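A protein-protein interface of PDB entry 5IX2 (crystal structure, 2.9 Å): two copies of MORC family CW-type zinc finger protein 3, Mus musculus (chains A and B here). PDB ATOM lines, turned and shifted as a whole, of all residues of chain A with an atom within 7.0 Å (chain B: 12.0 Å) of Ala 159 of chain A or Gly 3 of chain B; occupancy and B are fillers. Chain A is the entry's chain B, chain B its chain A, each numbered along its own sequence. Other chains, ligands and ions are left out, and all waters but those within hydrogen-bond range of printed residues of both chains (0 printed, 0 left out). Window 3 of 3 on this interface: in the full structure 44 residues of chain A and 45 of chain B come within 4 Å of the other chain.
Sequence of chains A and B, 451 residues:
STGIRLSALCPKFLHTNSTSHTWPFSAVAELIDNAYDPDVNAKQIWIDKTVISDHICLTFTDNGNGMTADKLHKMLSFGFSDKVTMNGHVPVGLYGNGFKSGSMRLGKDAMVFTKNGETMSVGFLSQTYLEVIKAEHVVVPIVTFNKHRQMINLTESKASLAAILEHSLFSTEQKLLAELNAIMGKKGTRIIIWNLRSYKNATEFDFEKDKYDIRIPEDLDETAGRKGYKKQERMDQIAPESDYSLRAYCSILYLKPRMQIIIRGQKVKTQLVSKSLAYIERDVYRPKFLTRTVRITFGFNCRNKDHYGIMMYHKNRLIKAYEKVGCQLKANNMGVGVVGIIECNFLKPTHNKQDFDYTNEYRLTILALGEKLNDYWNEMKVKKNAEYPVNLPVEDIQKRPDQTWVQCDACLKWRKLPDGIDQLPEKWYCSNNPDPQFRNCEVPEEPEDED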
ATOM      1  N   TYR A 129     -30.244 -21.111 -12.023  1.00  0.00           N
ATOM      2  CA  TYR A 129     -28.945 -20.518 -11.886  1.00  0.00           C
ATOM      3  C   TYR A 129     -29.074 -19.062 -11.604  1.00  0.00           C
ATOM      4  O   TYR A 129     -28.454 -18.521 -10.716  1.00  0.00           O
ATOM      5  CB  TYR A 129     -28.286 -20.629 -13.233  1.00  0.00           C
ATOM      6  CG  TYR A 129     -27.018 -19.861 -13.417  1.00  0.00           C
ATOM      7  CD1 TYR A 129     -26.111 -19.737 -12.409  1.00  0.00           C
ATOM      8  CD2 TYR A 129     -26.715 -19.299 -14.623  1.00  0.00           C
ATOM      9  CE1 TYR A 129     -24.938 -19.064 -12.595  1.00  0.00           C
ATOM     10  CE2 TYR A 129     -25.546 -18.624 -14.814  1.00  0.00           C
ATOM     11  CZ  TYR A 129     -24.667 -18.517 -13.795  1.00  0.00           C
ATOM     12  OH  TYR A 129     -23.513 -17.833 -14.002  1.00  0.00           O
ATOM     13  N   PRO A 141     -24.047 -18.418 -19.780  1.00  0.00           N
ATOM     14  CA  PRO A 141     -22.665 -18.895 -19.940  1.00  0.00           C
ATOM     15  C   PRO A 141     -22.399 -19.799 -21.124  1.00  0.00           C
ATOM     16  O   PRO A 141     -23.209 -20.611 -21.497  1.00  0.00           O
ATOM     17  CB  PRO A 141     -22.405 -19.683 -18.669  1.00  0.00           C
ATOM     18  CG  PRO A 141     -23.280 -19.081 -17.671  1.00  0.00           C
ATOM     19  CD  PRO A 141     -24.533 -18.965 -18.422  1.00  0.00           C
ATOM     20  N   ILE A 142     -21.229 -19.657 -21.709  1.00  0.00           N
ATOM     21  CA  ILE A 142     -20.874 -20.441 -22.856  1.00  0.00           C
ATOM     22  C   ILE A 142     -19.442 -20.877 -22.717  1.00  0.00           C
ATOM     23  O   ILE A 142     -18.627 -20.143 -22.210  1.00  0.00           O
ATOM     24  CB  ILE A 142     -21.055 -19.623 -24.117  1.00  0.00           C
ATOM     25  CG1 ILE A 142     -22.531 -19.377 -24.324  1.00  0.00           C
ATOM     26  CG2 ILE A 142     -20.494 -20.336 -25.311  1.00  0.00           C
ATOM     27  CD1 ILE A 142     -22.864 -18.672 -25.607  1.00  0.00           C
ATOM     28  N   VAL A 143     -19.145 -22.084 -23.177  1.00  0.00           N
ATOM     29  CA  VAL A 143     -17.810 -22.644 -23.095  1.00  0.00           C
ATOM     30  C   VAL A 143     -17.457 -23.180 -24.449  1.00  0.00           C
ATOM     31  O   VAL A 143     -18.311 -23.691 -25.126  1.00  0.00           O
ATOM     32  CB  VAL A 143     -17.763 -23.804 -22.117  1.00  0.00           C
ATOM     33  CG1 VAL A 143     -16.353 -24.034 -21.661  1.00  0.00           C
ATOM     34  CG2 VAL A 143     -18.638 -23.526 -20.920  1.00  0.00           C
ATOM     35  N   MET A 151      -9.819 -25.935 -24.609  1.00  0.00           N
ATOM     36  CA  MET A 151     -10.584 -24.740 -24.276  1.00  0.00           C
ATOM     37  C   MET A 151     -10.045 -23.515 -24.984  1.00  0.00           C
ATOM     38  O   MET A 151      -8.863 -23.408 -25.223  1.00  0.00           O
ATOM     39  CB  MET A 151     -10.550 -24.529 -22.767  1.00  0.00           C
ATOM     40  CG  MET A 151     -11.397 -23.393 -22.246  1.00  0.00           C
ATOM     41  SD  MET A 151     -12.491 -23.926 -20.932  1.00  0.00           S
ATOM     42  CE  MET A 151     -11.719 -23.225 -19.501  1.00  0.00           C
ATOM     43  N   LEU A 154     -10.816 -17.972 -23.878  1.00  0.00           N
ATOM     44  CA  LEU A 154     -10.518 -18.428 -22.552  1.00  0.00           C
ATOM     45  C   LEU A 154     -11.138 -17.614 -21.459  1.00  0.00           C
ATOM     46  O   LEU A 154     -11.535 -18.167 -20.440  1.00  0.00           O
ATOM     47  CB  LEU A 154      -9.011 -18.433 -22.362  1.00  0.00           C
ATOM     48  CG  LEU A 154      -8.209 -18.730 -23.632  1.00  0.00           C
ATOM     49  CD1 LEU A 154      -8.797 -19.952 -24.310  1.00  0.00           C
ATOM     50  CD2 LEU A 154      -8.217 -17.541 -24.588  1.00  0.00           C
ATOM     51  N   THR A 155     -11.185 -16.306 -21.631  1.00  0.00           N
ATOM     52  CA  THR A 155     -11.658 -15.475 -20.554  1.00  0.00           C
ATOM     53  C   THR A 155     -13.083 -15.851 -20.256  1.00  0.00           C
ATOM     54  O   THR A 155     -13.427 -16.101 -19.113  1.00  0.00           O
ATOM     55  CB  THR A 155     -11.690 -14.027 -21.010  1.00  0.00           C
ATOM     56  OG1 THR A 155     -12.623 -13.911 -22.084  1.00  0.00           O
ATOM     57  CG2 THR A 155     -10.346 -13.622 -21.520  1.00  0.00           C
ATOM     58  N   GLU A 156     -13.896 -15.937 -21.302  1.00  0.00           N
ATOM     59  CA  GLU A 156     -15.306 -16.281 -21.160  1.00  0.00           C
ATOM     60  C   GLU A 156     -15.551 -17.697 -20.711  1.00  0.00           C
ATOM     61  O   GLU A 156     -16.404 -17.964 -19.879  1.00  0.00           O
ATOM     62  CB  GLU A 156     -16.063 -16.037 -22.455  1.00  0.00           C
ATOM     63  CG  GLU A 156     -17.533 -16.351 -22.315  1.00  0.00           C
ATOM     64  CD  GLU A 156     -18.283 -16.269 -23.613  1.00  0.00           C
ATOM     65  OE1 GLU A 156     -17.649 -16.247 -24.675  1.00  0.00           O
ATOM     66  OE2 GLU A 156     -19.516 -16.221 -23.560  1.00  0.00           O
ATOM     67  N   SER A 157     -14.800 -18.611 -21.296  1.00  0.00           N
ATOM     68  CA  SER A 157     -14.973 -20.002 -21.006  1.00  0.00           C
ATOM     69  C   SER A 157     -14.637 -20.265 -19.571  1.00  0.00           C
ATOM     70  O   SER A 157     -15.333 -21.003 -18.895  1.00  0.00           O
ATOM     71  CB  SER A 157     -14.094 -20.806 -21.927  1.00  0.00           C
ATOM     72  OG  SER A 157     -14.256 -20.330 -23.241  1.00  0.00           O
ATOM     73  N   LYS A 158     -13.583 -19.635 -19.092  1.00  0.00           N
ATOM     74  CA  LYS A 158     -13.120 -19.946 -17.772  1.00  0.00           C
ATOM     75  C   LYS A 158     -14.212 -19.618 -16.796  1.00  0.00           C
ATOM     76  O   LYS A 158     -14.544 -20.423 -15.957  1.00  0.00           O
ATOM     77  CB  LYS A 158     -11.874 -19.133 -17.462  1.00  0.00           C
ATOM     78  CG  LYS A 158     -11.262 -19.413 -16.102  1.00  0.00           C
ATOM     79  CD  LYS A 158     -10.202 -18.380 -15.750  1.00  0.00           C
ATOM     80  CE  LYS A 158     -10.475 -17.724 -14.403  1.00  0.00           C
ATOM     81  NZ  LYS A 158      -9.701 -16.464 -14.204  1.00  0.00           N
ATOM     82  N   ALA A 159     -14.810 -18.451 -16.930  1.00  0.00           N
ATOM     83  CA  ALA A 159     -15.884 -18.077 -16.032  1.00  0.00           C
ATOM     84  C   ALA A 159     -17.090 -18.940 -16.226  1.00  0.00           C
ATOM     85  O   ALA A 159     -17.750 -19.331 -15.287  1.00  0.00           O
ATOM     86  CB  ALA A 159     -16.250 -16.629 -16.221  1.00  0.00           C
ATOM     87  N   SER A 160     -17.406 -19.169 -17.479  1.00  0.00           N
ATOM     88  CA  SER A 160     -18.592 -19.884 -17.814  1.00  0.00           C
ATOM     89  C   SER A 160     -18.498 -21.277 -17.290  1.00  0.00           C
ATOM     90  O   SER A 160     -19.425 -21.786 -16.696  1.00  0.00           O
ATOM     91  CB  SER A 160     -18.704 -19.887 -19.315  1.00  0.00           C
ATOM     92  OG  SER A 160     -18.967 -18.567 -19.744  1.00  0.00           O
ATOM     93  N   LEU A 161     -17.348 -21.887 -17.468  1.00  0.00           N
ATOM     94  CA  LEU A 161     -17.194 -23.261 -17.097  1.00  0.00           C
ATOM     95  C   LEU A 161     -17.372 -23.433 -15.619  1.00  0.00           C
ATOM     96  O   LEU A 161     -18.002 -24.361 -15.167  1.00  0.00           O
ATOM     97  CB  LEU A 161     -15.831 -23.734 -17.511  1.00  0.00           C
ATOM     98  CG  LEU A 161     -15.521 -25.167 -17.131  1.00  0.00           C
ATOM     99  CD1 LEU A 161     -16.524 -26.099 -17.761  1.00  0.00           C
ATOM    100  CD2 LEU A 161     -14.137 -25.506 -17.617  1.00  0.00           C
ATOM    101  N   ALA A 162     -16.817 -22.521 -14.858  1.00  0.00           N
ATOM    102  CA  ALA A 162     -16.906 -22.611 -13.427  1.00  0.00           C
ATOM    103  C   ALA A 162     -18.346 -22.517 -13.063  1.00  0.00           C
ATOM    104  O   ALA A 162     -18.811 -23.159 -12.149  1.00  0.00           O
ATOM    105  CB  ALA A 162     -16.155 -21.472 -12.799  1.00  0.00           C
ATOM    106  N   ALA A 163     -19.043 -21.644 -13.755  1.00  0.00           N
ATOM    107  CA  ALA A 163     -20.437 -21.432 -13.492  1.00  0.00           C
ATOM    108  C   ALA A 163     -21.231 -22.655 -13.808  1.00  0.00           C
ATOM    109  O   ALA A 163     -22.123 -23.034 -13.078  1.00  0.00           O
ATOM    110  CB  ALA A 163     -20.919 -20.291 -14.334  1.00  0.00           C
ATOM    111  N   ILE A 164     -20.915 -23.265 -14.933  1.00  0.00           N
ATOM    112  CA  ILE A 164     -21.626 -24.446 -15.328  1.00  0.00           C
ATOM    113  C   ILE A 164     -21.373 -25.538 -14.346  1.00  0.00           C
ATOM    114  O   ILE A 164     -22.292 -26.157 -13.873  1.00  0.00           O
ATOM    115  CB  ILE A 164     -21.144 -24.927 -16.689  1.00  0.00           C
ATOM    116  CG1 ILE A 164     -21.318 -23.801 -17.703  1.00  0.00           C
ATOM    117  CG2 ILE A 164     -21.837 -26.218 -17.072  1.00  0.00           C
ATOM    118  CD1 ILE A 164     -21.826 -24.190 -19.070  1.00  0.00           C
ATOM    119  N   LEU A 165     -20.119 -25.737 -13.994  1.00  0.00           N
ATOM    120  CA  LEU A 165     -19.780 -26.886 -13.215  1.00  0.00           C
ATOM    121  C   LEU A 165     -20.490 -26.780 -11.905  1.00  0.00           C
ATOM    122  O   LEU A 165     -21.027 -27.751 -11.421  1.00  0.00           O
ATOM    123  CB  LEU A 165     -18.288 -26.956 -13.015  1.00  0.00           C
ATOM    124  CG  LEU A 165     -17.534 -27.292 -14.284  1.00  0.00           C
ATOM    125  CD1 LEU A 165     -16.067 -27.463 -13.989  1.00  0.00           C
ATOM    126  CD2 LEU A 165     -18.079 -28.583 -14.822  1.00  0.00           C
ATOM    127  N   GLY B   3     -16.445 -12.749 -17.116  1.00  0.00           N
ATOM    128  CA  GLY B   3     -16.321 -12.674 -18.555  1.00  0.00           C
ATOM    129  C   GLY B   3     -17.547 -13.207 -19.246  1.00  0.00           C
ATOM    130  O   GLY B   3     -17.630 -13.209 -20.459  1.00  0.00           O
ATOM    131  N   ILE B   4     -18.502 -13.657 -18.453  1.00  0.00           N
ATOM    132  CA  ILE B   4     -19.737 -14.190 -18.974  1.00  0.00           C
ATOM    133  C   ILE B   4     -20.564 -13.157 -19.686  1.00  0.00           C
ATOM    134  O   ILE B   4     -20.767 -12.078 -19.191  1.00  0.00           O
ATOM    135  CB  ILE B   4     -20.602 -14.703 -17.843  1.00  0.00           C
ATOM    136  CG1 ILE B   4     -19.817 -15.690 -17.013  1.00  0.00           C
ATOM    137  CG2 ILE B   4     -21.852 -15.348 -18.393  1.00  0.00           C
ATOM    138  CD1 ILE B   4     -20.669 -16.463 -16.048  1.00  0.00           C
ATOM    139  N   ARG B   5     -21.098 -13.529 -20.827  1.00  0.00           N
ATOM    140  CA  ARG B   5     -21.913 -12.640 -21.610  1.00  0.00           C
ATOM    141  C   ARG B   5     -23.322 -12.481 -21.111  1.00  0.00           C
ATOM    142  O   ARG B   5     -23.805 -13.267 -20.328  1.00  0.00           O
ATOM    143  CB  ARG B   5     -21.943 -13.100 -23.039  1.00  0.00           C
ATOM    144  CG  ARG B   5     -20.972 -12.336 -23.879  1.00  0.00           C
ATOM    145  CD  ARG B   5     -20.326 -13.215 -24.904  1.00  0.00           C
ATOM    146  NE  ARG B   5     -20.729 -12.817 -26.231  1.00  0.00           N
ATOM    147  CZ  ARG B   5     -20.721 -11.573 -26.665  1.00  0.00           C
ATOM    148  NH1 ARG B   5     -21.106 -11.299 -27.894  1.00  0.00           N
ATOM    149  NH2 ARG B   5     -20.301 -10.609 -25.877  1.00  0.00           N
ATOM    150  N   LEU B   6     -23.977 -11.437 -21.576  1.00  0.00           N
ATOM    151  CA  LEU B   6     -25.356 -11.219 -21.265  1.00  0.00           C
ATOM    152  C   LEU B   6     -26.110 -11.577 -22.472  1.00  0.00           C
ATOM    153  O   LEU B   6     -25.626 -11.426 -23.562  1.00  0.00           O
ATOM    154  CB  LEU B   6     -25.630  -9.760 -21.052  1.00  0.00           C
ATOM    155  CG  LEU B   6     -24.891  -9.010 -19.986  1.00  0.00           C
ATOM    156  CD1 LEU B   6     -24.509  -7.699 -20.618  1.00  0.00           C
ATOM    157  CD2 LEU B   6     -25.819  -8.762 -18.827  1.00  0.00           C
ATOM    158  N   SER B   7     -27.324 -12.028 -22.277  1.00  0.00           N
ATOM    159  CA  SER B   7     -28.195 -12.249 -23.386  1.00  0.00           C
ATOM    160  C   SER B   7     -28.488 -10.896 -23.949  1.00  0.00           C
ATOM    161  O   SER B   7     -28.440  -9.926 -23.245  1.00  0.00           O
ATOM    162  CB  SER B   7     -29.465 -12.908 -22.925  1.00  0.00           C
ATOM    163  OG  SER B   7     -30.015 -13.631 -23.985  1.00  0.00           O
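Among the printed residues, merely in contact across the chains: Glu 156 of chain A with Arg 5 of chain B, Glu 156 of chain A with Gly 3 of chain B, Tyr 129 of chain A with Ile 4 of chain B, Ala 159 of chain A with Ile 4 of chain B, Pro 141 of chain A with Ile 4 of chain B and Ala 159 of chain A with Gly 3 of chain B.
No position is printed for both chains.
Of the 6 pairs that touch across the chains among the printed residues, none has its exchanged pair printed and touching as well.
Printed residues of chain B within 4 Å of Ala 159 of chain A: Gly 3 and Ile 4.
Of the printed residues of chain A, Gly 3 of chain B touches Glu 156 and Ala 159.
No residue of chain B comes within 4 Å of Thr 155 of chain A.
Glu 156 of chain A touches two residues of chain B.
No residue of chain B comes within 4 Å of Ser 157 of chain A.
No residue of chain B comes within 4 Å of Ala 162 of chain A.
Printed residues of chain A within 4 Å of Ile 4 of chain B: Tyr 129 (3.8 Å), Pro 141 (3.95 Å) and Ala 159 (3.8 Å).
Printed residues of chain B within 4 Å of Pro 141 of chain A: Ile 4.
The nearest printed residue of chain B that does not touch Ala 159 of chain A is Arg 5 of chain B (7.4 Å).
The side-chain hydroxyl (OG) of Ser 160 of chain A is in hydrogen-bond range of the backbone carbonyl oxygen (O) of Glu 156 of chain A.
Of the 17 printed residues of chain A, 4 touch a printed residue of chain B.
Printed residues of chain A that touch a printed residue of chain B: Tyr 129, Pro 141, Glu 156 and Ala 159.
Hydrophobic or aromatic side chains of chain A that line the printed part of chain B: Tyr 129 and Ala 159.
Printed residues of chain B that touch a printed residue of chain A: Gly 3, Ile 4 and Arg 5.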
